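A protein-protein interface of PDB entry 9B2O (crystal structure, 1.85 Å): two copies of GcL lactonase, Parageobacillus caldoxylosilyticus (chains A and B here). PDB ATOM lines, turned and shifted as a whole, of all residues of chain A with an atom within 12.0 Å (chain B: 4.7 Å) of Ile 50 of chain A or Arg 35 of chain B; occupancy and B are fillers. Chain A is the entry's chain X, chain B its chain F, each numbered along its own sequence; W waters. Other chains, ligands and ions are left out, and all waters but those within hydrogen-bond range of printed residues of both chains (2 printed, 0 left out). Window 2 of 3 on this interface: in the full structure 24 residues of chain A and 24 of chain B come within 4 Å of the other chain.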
ATOM      1  N   MET A  44      15.690  -0.033   2.952  1.00  0.00           N
ATOM      2  CA  MET A  44      16.356  -0.466   1.692  1.00  0.00           C
ATOM      3  C   MET A  44      15.514  -1.522   0.994  1.00  0.00           C
ATOM      4  O   MET A  44      16.055  -2.544   0.557  1.00  0.00           O
ATOM      5  CB  MET A  44      17.751  -1.026   1.984  1.00  0.00           C
ATOM      6  CG  MET A  44      18.653  -0.048   2.672  1.00  0.00           C
ATOM      7  SD  MET A  44      18.907   1.582   1.851  1.00  0.00           S
ATOM      8  CE  MET A  44      19.253   0.974   0.196  1.00  0.00           C
ATOM      9  N   ASN A  46      14.093  -1.468  -1.855  1.00  0.00           N
ATOM     10  CA  ASN A  46      14.231  -1.502  -3.341  1.00  0.00           C
ATOM     11  C   ASN A  46      15.504  -0.743  -3.726  1.00  0.00           C
ATOM     12  O   ASN A  46      15.458   0.350  -4.296  1.00  0.00           O
ATOM     13  CB  ASN A  46      12.952  -0.989  -4.009  1.00  0.00           C
ATOM     14  CG  ASN A  46      13.008  -1.061  -5.523  1.00  0.00           C
ATOM     15  OD1 ASN A  46      13.601  -1.978  -6.078  1.00  0.00           O
ATOM     16  ND2 ASN A  46      12.491  -0.044  -6.190  1.00  0.00           N
ATOM     17  N   PRO A  47      16.692  -1.304  -3.420  1.00  0.00           N
ATOM     18  CA  PRO A  47      17.946  -0.580  -3.622  1.00  0.00           C
ATOM     19  C   PRO A  47      18.219  -0.306  -5.111  1.00  0.00           C
ATOM     20  O   PRO A  47      17.951  -1.144  -5.928  1.00  0.00           O
ATOM     21  CB  PRO A  47      19.026  -1.515  -3.064  1.00  0.00           C
ATOM     22  CG  PRO A  47      18.241  -2.536  -2.209  1.00  0.00           C
ATOM     23  CD  PRO A  47      16.903  -2.671  -2.907  1.00  0.00           C
ATOM     24  N   ALA A  48      18.756   0.865  -5.416  1.00  0.00           N
ATOM     25  CA  ALA A  48      19.313   1.197  -6.739  1.00  0.00           C
ATOM     26  C   ALA A  48      20.327   0.133  -7.165  1.00  0.00           C
ATOM     27  O   ALA A  48      21.053  -0.461  -6.302  1.00  0.00           O
ATOM     28  CB  ALA A  48      19.907   2.585  -6.715  1.00  0.00           C
ATOM     29  N   THR A  49      20.375  -0.124  -8.471  1.00  0.00           N
ATOM     30  CA  THR A  49      21.306  -1.061  -9.154  1.00  0.00           C
ATOM     31  C   THR A  49      21.861  -0.334 -10.400  1.00  0.00           C
ATOM     32  O   THR A  49      21.365   0.763 -10.748  1.00  0.00           O
ATOM     33  CB  THR A  49      20.636  -2.387  -9.565  1.00  0.00           C
ATOM     34  OG1 THR A  49      19.575  -2.049 -10.458  1.00  0.00           O
ATOM     35  CG2 THR A  49      20.070  -3.200  -8.423  1.00  0.00           C
ATOM     36  N   ILE A  50      22.921  -0.886 -10.971  1.00  0.00           N
ATOM     37  CA  ILE A  50      23.523  -0.409 -12.248  1.00  0.00           C
ATOM     38  C   ILE A  50      22.382  -0.276 -13.289  1.00  0.00           C
ATOM     39  O   ILE A  50      22.279   0.810 -13.893  1.00  0.00           O
ATOM     40  CB  ILE A  50      24.691  -1.350 -12.621  1.00  0.00           C
ATOM     41  CG1 ILE A  50      25.654  -0.702 -13.620  1.00  0.00           C
ATOM     42  CG2 ILE A  50      24.176  -2.707 -13.083  1.00  0.00           C
ATOM     43  CD1 ILE A  50      26.909  -1.517 -13.907  1.00  0.00           C
ATOM     44  N   HIS A  51      21.430  -1.219 -13.342  1.00  0.00           N
ATOM     45  CA  HIS A  51      20.275  -1.202 -14.285  1.00  0.00           C
ATOM     46  C   HIS A  51      19.163  -0.259 -13.803  1.00  0.00           C
ATOM     47  O   HIS A  51      18.435   0.257 -14.669  1.00  0.00           O
ATOM     48  CB  HIS A  51      19.836  -2.638 -14.625  1.00  0.00           C
ATOM     49  CG  HIS A  51      20.874  -3.326 -15.461  1.00  0.00           C
ATOM     50  ND1 HIS A  51      21.518  -4.497 -15.050  1.00  0.00           N
ATOM     51  CD2 HIS A  51      21.458  -2.967 -16.634  1.00  0.00           C
ATOM     52  CE1 HIS A  51      22.413  -4.850 -15.955  1.00  0.00           C
ATOM     53  NE2 HIS A  51      22.391  -3.928 -16.942  1.00  0.00           N
ATOM     54  N   ASN A  52      19.043   0.027 -12.501  1.00  0.00           N
ATOM     55  CA  ASN A  52      17.981   0.928 -11.973  1.00  0.00           C
ATOM     56  C   ASN A  52      18.628   1.936 -11.026  1.00  0.00           C
ATOM     57  O   ASN A  52      18.383   1.909  -9.817  1.00  0.00           O
ATOM     58  CB  ASN A  52      16.808   0.130 -11.373  1.00  0.00           C
ATOM     59  CG  ASN A  52      15.602   0.987 -11.045  1.00  0.00           C
ATOM     60  OD1 ASN A  52      15.440   2.066 -11.610  1.00  0.00           O
ATOM     61  ND2 ASN A  52      14.787   0.563 -10.088  1.00  0.00           N
ATOM     62  N   PRO A  53      19.480   2.854 -11.552  1.00  0.00           N
ATOM     63  CA  PRO A  53      20.332   3.700 -10.712  1.00  0.00           C
ATOM     64  C   PRO A  53      19.566   4.830 -10.003  1.00  0.00           C
ATOM     65  O   PRO A  53      20.080   5.407  -9.020  1.00  0.00           O
ATOM     66  CB  PRO A  53      21.392   4.240 -11.700  1.00  0.00           C
ATOM     67  CG  PRO A  53      20.674   4.243 -13.045  1.00  0.00           C
ATOM     68  CD  PRO A  53      19.763   3.031 -12.993  1.00  0.00           C
ATOM     69  N   ASN A  54      18.360   5.118 -10.472  1.00  0.00           N
ATOM     70  CA  ASN A  54      17.480   6.155  -9.871  1.00  0.00           C
ATOM     71  C   ASN A  54      16.214   5.501  -9.338  1.00  0.00           C
ATOM     72  O   ASN A  54      15.129   6.088  -9.511  1.00  0.00           O
ATOM     73  CB  ASN A  54      17.141   7.252 -10.874  1.00  0.00           C
ATOM     74  CG  ASN A  54      18.398   7.884 -11.421  1.00  0.00           C
ATOM     75  OD1 ASN A  54      19.224   8.373 -10.655  1.00  0.00           O
ATOM     76  ND2 ASN A  54      18.568   7.835 -12.727  1.00  0.00           N
ATOM     77  N   ALA A  55      16.358   4.334  -8.714  1.00  0.00           N
ATOM     78  CA  ALA A  55      15.224   3.535  -8.195  1.00  0.00           C
ATOM     79  C   ALA A  55      14.261   4.450  -7.454  1.00  0.00           C
ATOM     80  O   ALA A  55      14.708   5.365  -6.699  1.00  0.00           O
ATOM     81  CB  ALA A  55      15.669   2.408  -7.313  1.00  0.00           C
ATOM     82  N   GLN A  56      12.986   4.180  -7.680  1.00  0.00           N
ATOM     83  CA  GLN A  56      11.857   4.917  -7.080  1.00  0.00           C
ATOM     84  C   GLN A  56      11.385   4.159  -5.846  1.00  0.00           C
ATOM     85  O   GLN A  56      11.335   2.897  -5.847  1.00  0.00           O
ATOM     86  CB  GLN A  56      10.705   5.056  -8.077  1.00  0.00           C
ATOM     87  CG  GLN A  56      10.974   6.156  -9.087  1.00  0.00           C
ATOM     88  CD  GLN A  56       9.947   6.124 -10.189  1.00  0.00           C
ATOM     89  OE1 GLN A  56       8.770   5.836  -9.953  1.00  0.00           O
ATOM     90  NE2 GLN A  56      10.419   6.357 -11.402  1.00  0.00           N
ATOM     91  N   ARG B  33      37.032   2.621  -7.626  1.00  0.00           N
ATOM     92  CA  ARG B  33      35.772   3.354  -7.361  1.00  0.00           C
ATOM     93  C   ARG B  33      34.634   2.328  -7.268  1.00  0.00           C
ATOM     94  O   ARG B  33      34.621   1.303  -8.012  1.00  0.00           O
ATOM     95  CB  ARG B  33      35.472   4.368  -8.472  1.00  0.00           C
ATOM     96  CG  ARG B  33      36.556   5.404  -8.722  1.00  0.00           C
ATOM     97  CD  ARG B  33      36.586   6.528  -7.712  1.00  0.00           C
ATOM     98  NE  ARG B  33      37.749   7.397  -7.922  1.00  0.00           N
ATOM     99  CZ  ARG B  33      39.018   7.088  -7.592  1.00  0.00           C
ATOM    100  NH1 ARG B  33      39.321   5.942  -6.991  1.00  0.00           N
ATOM    101  NH2 ARG B  33      39.991   7.949  -7.849  1.00  0.00           N
ATOM    102  N   MET B  34      33.694   2.590  -6.380  1.00  0.00           N
ATOM    103  CA  MET B  34      32.448   1.813  -6.247  1.00  0.00           C
ATOM    104  C   MET B  34      31.273   2.770  -6.397  1.00  0.00           C
ATOM    105  O   MET B  34      31.414   4.011  -6.139  1.00  0.00           O
ATOM    106  CB  MET B  34      32.449   1.114  -4.888  1.00  0.00           C
ATOM    107  CG  MET B  34      31.247   0.255  -4.625  1.00  0.00           C
ATOM    108  SD  MET B  34      31.494  -0.755  -3.108  1.00  0.00           S
ATOM    109  CE  MET B  34      32.751  -1.927  -3.620  1.00  0.00           C
ATOM    110  N   ARG B  35      30.140   2.226  -6.807  1.00  0.00           N
ATOM    111  CA  ARG B  35      28.874   2.963  -6.787  1.00  0.00           C
ATOM    112  C   ARG B  35      27.878   2.142  -5.980  1.00  0.00           C
ATOM    113  O   ARG B  35      27.962   0.876  -6.013  1.00  0.00           O
ATOM    114  CB  ARG B  35      28.381   3.192  -8.214  1.00  0.00           C
ATOM    115  CG  ARG B  35      29.332   4.037  -9.052  1.00  0.00           C
ATOM    116  CD  ARG B  35      28.823   4.219 -10.479  1.00  0.00           C
ATOM    117  NE  ARG B  35      28.930   2.988 -11.270  1.00  0.00           N
ATOM    118  CZ  ARG B  35      28.138   2.674 -12.323  1.00  0.00           C
ATOM    119  NH1 ARG B  35      27.198   3.511 -12.742  1.00  0.00           N
ATOM    120  NH2 ARG B  35      28.304   1.532 -12.958  1.00  0.00           N
ATOM    121  N   MET B  36      26.969   2.845  -5.327  1.00  0.00           N
ATOM    122  CA  MET B  36      25.780   2.204  -4.734  1.00  0.00           C
ATOM    123  C   MET B  36      24.707   3.261  -4.489  1.00  0.00           C
ATOM    124  O   MET B  36      25.010   4.470  -4.568  1.00  0.00           O
ATOM    125  CB  MET B  36      26.184   1.545  -3.417  1.00  0.00           C
ATOM    126  CG  MET B  36      26.576   2.552  -2.340  1.00  0.00           C
ATOM    127  SD  MET B  36      27.301   1.692  -0.895  1.00  0.00           S
ATOM    128  CE  MET B  36      27.582   3.124   0.141  1.00  0.00           C
ATOM    129  N   PHE B  59      22.715   7.005  -7.640  1.00  0.00           N
ATOM    130  CA  PHE B  59      23.692   5.896  -7.630  1.00  0.00           C
ATOM    131  C   PHE B  59      25.059   6.567  -7.561  1.00  0.00           C
ATOM    132  O   PHE B  59      25.516   7.060  -8.624  1.00  0.00           O
ATOM    133  CB  PHE B  59      23.473   5.025  -8.865  1.00  0.00           C
ATOM    134  CG  PHE B  59      23.971   3.609  -8.797  1.00  0.00           C
ATOM    135  CD1 PHE B  59      23.529   2.742  -7.808  1.00  0.00           C
ATOM    136  CD2 PHE B  59      24.868   3.128  -9.737  1.00  0.00           C
ATOM    137  CE1 PHE B  59      23.961   1.425  -7.774  1.00  0.00           C
ATOM    138  CE2 PHE B  59      25.318   1.815  -9.690  1.00  0.00           C
ATOM    139  CZ  PHE B  59      24.863   0.964  -8.706  1.00  0.00           C
ATOM    140  N   VAL B  60      25.632   6.684  -6.358  1.00  0.00           N
ATOM    141  CA  VAL B  60      26.751   7.632  -6.086  1.00  0.00           C
ATOM    142  C   VAL B  60      28.069   6.878  -6.124  1.00  0.00           C
ATOM    143  O   VAL B  60      28.117   5.695  -5.769  1.00  0.00           O
ATOM    144  CB  VAL B  60      26.611   8.394  -4.756  1.00  0.00           C
ATOM    145  CG1 VAL B  60      25.477   9.391  -4.798  1.00  0.00           C
ATOM    146  CG2 VAL B  60      26.469   7.451  -3.569  1.00  0.00           C
ATOM    147  N   GLU B  61      29.101   7.575  -6.581  1.00  0.00           N
ATOM    148  CA  GLU B  61      30.451   7.022  -6.810  1.00  0.00           C
ATOM    149  C   GLU B  61      31.377   7.420  -5.660  1.00  0.00           C
ATOM    150  O   GLU B  61      31.342   8.558  -5.201  1.00  0.00           O
ATOM    151  CB  GLU B  61      31.030   7.492  -8.153  1.00  0.00           C
ATOM    152  CG  GLU B  61      32.249   6.662  -8.523  1.00  0.00           C
ATOM    153  CD  GLU B  61      33.007   7.004  -9.796  1.00  0.00           C
ATOM    154  OE1 GLU B  61      33.659   8.063  -9.855  1.00  0.00           O
ATOM    155  OE2 GLU B  61      33.008   6.149 -10.674  1.00  0.00           O
ATOM    156  N   PHE B  62      32.250   6.519  -5.239  1.00  0.00           N
ATOM    157  CA  PHE B  62      33.132   6.794  -4.085  1.00  0.00           C
ATOM    158  C   PHE B  62      34.404   5.964  -4.223  1.00  0.00           C
ATOM    159  O   PHE B  62      34.407   4.898  -4.828  1.00  0.00           O
ATOM    160  CB  PHE B  62      32.339   6.574  -2.779  1.00  0.00           C
ATOM    161  CG  PHE B  62      31.807   5.183  -2.576  1.00  0.00           C
ATOM    162  CD1 PHE B  62      32.585   4.186  -2.003  1.00  0.00           C
ATOM    163  CD2 PHE B  62      30.528   4.857  -2.995  1.00  0.00           C
ATOM    164  CE1 PHE B  62      32.081   2.902  -1.811  1.00  0.00           C
ATOM    165  CE2 PHE B  62      30.031   3.578  -2.812  1.00  0.00           C
ATOM    166  CZ  PHE B  62      30.808   2.598  -2.233  1.00  0.00           C
ATOM    167  N   GLN B  99      25.757  -6.009  -8.987  1.00  0.00           N
ATOM    168  CA  GLN B  99      24.778  -5.037  -9.546  1.00  0.00           C
ATOM    169  C   GLN B  99      24.472  -3.903  -8.547  1.00  0.00           C
ATOM    170  O   GLN B  99      24.174  -2.770  -9.001  1.00  0.00           O
ATOM    171  CB  GLN B  99      23.525  -5.795 -10.004  1.00  0.00           C
ATOM    172  CG  GLN B  99      23.778  -6.643 -11.252  1.00  0.00           C
ATOM    173  CD  GLN B  99      22.510  -7.077 -11.953  1.00  0.00           C
ATOM    174  OE1 GLN B  99      22.356  -8.241 -12.321  1.00  0.00           O
ATOM    175  NE2 GLN B  99      21.590  -6.144 -12.160  1.00  0.00           N
ATOM    176  N   MET B 100      24.525  -4.150  -7.237  1.00  0.00           N
ATOM    177  CA  MET B 100      24.203  -3.099  -6.234  1.00  0.00           C
ATOM    178  C   MET B 100      25.459  -2.312  -5.815  1.00  0.00           C
ATOM    179  O   MET B 100      25.298  -1.166  -5.362  1.00  0.00           O
ATOM    180  CB  MET B 100      23.585  -3.704  -4.964  1.00  0.00           C
ATOM    181  CG  MET B 100      22.113  -3.914  -5.045  1.00  0.00           C
ATOM    182  SD  MET B 100      21.421  -4.534  -3.465  1.00  0.00           S
ATOM    183  CE  MET B 100      22.077  -6.203  -3.388  1.00  0.00           C
ATOM    184  N   PHE B 101      26.638  -2.916  -5.884  1.00  0.00           N
ATOM    185  CA  PHE B 101      27.927  -2.375  -5.365  1.00  0.00           C
ATOM    186  C   PHE B 101      29.050  -2.568  -6.389  1.00  0.00           C
ATOM    187  O   PHE B 101      30.142  -2.998  -6.045  1.00  0.00           O
ATOM    188  CB  PHE B 101      28.329  -3.070  -4.056  1.00  0.00           C
ATOM    189  CG  PHE B 101      27.230  -3.073  -3.030  1.00  0.00           C
ATOM    190  CD1 PHE B 101      26.919  -1.929  -2.326  1.00  0.00           C
ATOM    191  CD2 PHE B 101      26.481  -4.222  -2.802  1.00  0.00           C
ATOM    192  CE1 PHE B 101      25.887  -1.937  -1.399  1.00  0.00           C
ATOM    193  CE2 PHE B 101      25.455  -4.229  -1.870  1.00  0.00           C
ATOM    194  CZ  PHE B 101      25.156  -3.081  -1.173  1.00  0.00           C
ATOM    195  N   PRO B 102      28.821  -2.226  -7.677  1.00  0.00           N
ATOM    196  CA  PRO B 102      29.841  -2.425  -8.701  1.00  0.00           C
ATOM    197  C   PRO B 102      31.156  -1.684  -8.394  1.00  0.00           C
ATOM    198  O   PRO B 102      31.174  -0.492  -8.079  1.00  0.00           O
ATOM    199  CB  PRO B 102      29.151  -1.902  -9.990  1.00  0.00           C
ATOM    200  CG  PRO B 102      28.129  -0.906  -9.472  1.00  0.00           C
ATOM    201  CD  PRO B 102      27.605  -1.553  -8.187  1.00  0.00           C
HETATM  202  O   HOH W   1      22.227   8.258 -10.139  1.00  0.00           O
HETATM  203  O   HOH W   2      23.089  -0.024  -4.436  1.00  0.00           O
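Among the printed residues, merely in contact across the chains: Pro 47 of chain A with Met 100 of chain B (3.9 Å), Ala 48 of chain A with Phe 59 of chain B (3.8 Å), Ala 48 of chain A with Met 100 of chain B (3.8 Å), Thr 49 of chain A with Phe 59 of chain B (3.7 Å), Thr 49 of chain A with Gln 99 of chain B (3.3 Å), Ile 50 of chain A with Arg 35 of chain B (3.5 Å) and Ile 50 of chain A with Phe 59 of chain B (3.5 Å).
A ring nitrogen (ND1) of His 51 of chain A lies within hydrogen-bond range of the side-chain amide nitrogen (NE2) of Gln 99 of chain B, at 3.3 Å. N of Phe 59 of chain B is in hydrogen-bond range of O of Pro 53 of chain A (3.4 Å). The backbone NH of Ile 50 of chain A is in hydrogen-bond range of the backbone carbonyl oxygen of Gln 99 of chain B, 3.0 Å away.
The side-chain hydroxyl of Thr 49 of chain A is in hydrogen-bond range of the backbone NH of Asn 52 of chain A (3.0 Å). O of Pro 102 of chain B sits at hydrogen-bond distance from N of Arg 35 of chain B (3.2 Å).
No position is printed for both chains.
Printed residues of chain B within 4 Å of Pro 47 of chain A: Met 100 (3.9 Å). Of the printed residues of chain B, Ala 48 of chain A touches Phe 59 (3.8 Å) and Met 100 (3.8 Å). Ile 50 of chain A touches just these residues of chain B: Arg 35, Phe 59 and Gln 99. Ala 55 of chain A touches none of the printed residues of chain B. No residue of chain A comes within 4 Å of Met 34 of chain B. Arg 35 of chain B touches just one residue of chain A: Ile 50 (3.5 Å). Of chain A, only Ala 48, Thr 49, Ile 50 and Pro 53 come within 4 Å of Phe 59 of chain B. No residue of chain A comes within 4 Å of Val 60 of chain B. No residue of chain A comes within 4 Å of Glu 61 of chain B. Phe 62 of chain B touches none of the printed residues of chain A. Of chain A, only Thr 49, Ile 50 and His 51 come within 4 Å of Gln 99 of chain B. Of the printed residues of chain A, Met 100 of chain B touches Pro 47 (3.9 Å) and Ala 48 (3.8 Å). No residue of chain A comes within 4 Å of Phe 101 of chain B. No residue of chain A comes within 4 Å of Pro 102 of chain B. The nearest residue of chain A that does not touch Arg 35 of chain B is Pro 53 of chain A (5.9 Å).
Printed residues of chain A that touch a printed residue of chain B: Pro 47, Ala 48, Thr 49, Ile 50, His 51 and Pro 53. Hydrophobic or aromatic side chains of chain A within 4 Å of the printed part of chain B: Pro 47, Ala 48, Ile 50, His 51 and Pro 53. Printed residues of chain B that touch a printed residue of chain A: Arg 35, Phe 59, Gln 99 and Met 100. Hydrophobic or aromatic side chains of chain B that line the printed part of chain A: Phe 59 and Met 100. Among the printed residues, 10 pairs touch across the chains. Among the printed residues, no Asp or Glu carboxylate lies within 4 Å of a Lys or Arg side-chain nitrogen of the other chain.
Water W2 bridges O of Met 100 of chain B (2.7 Å) and O of Ala 48 of chain A (2.8 Å). Water W1 bridges N of Phe 59 of chain B (2.8 Å) and OD1 of Asn 54 of chain A (3.0 Å).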
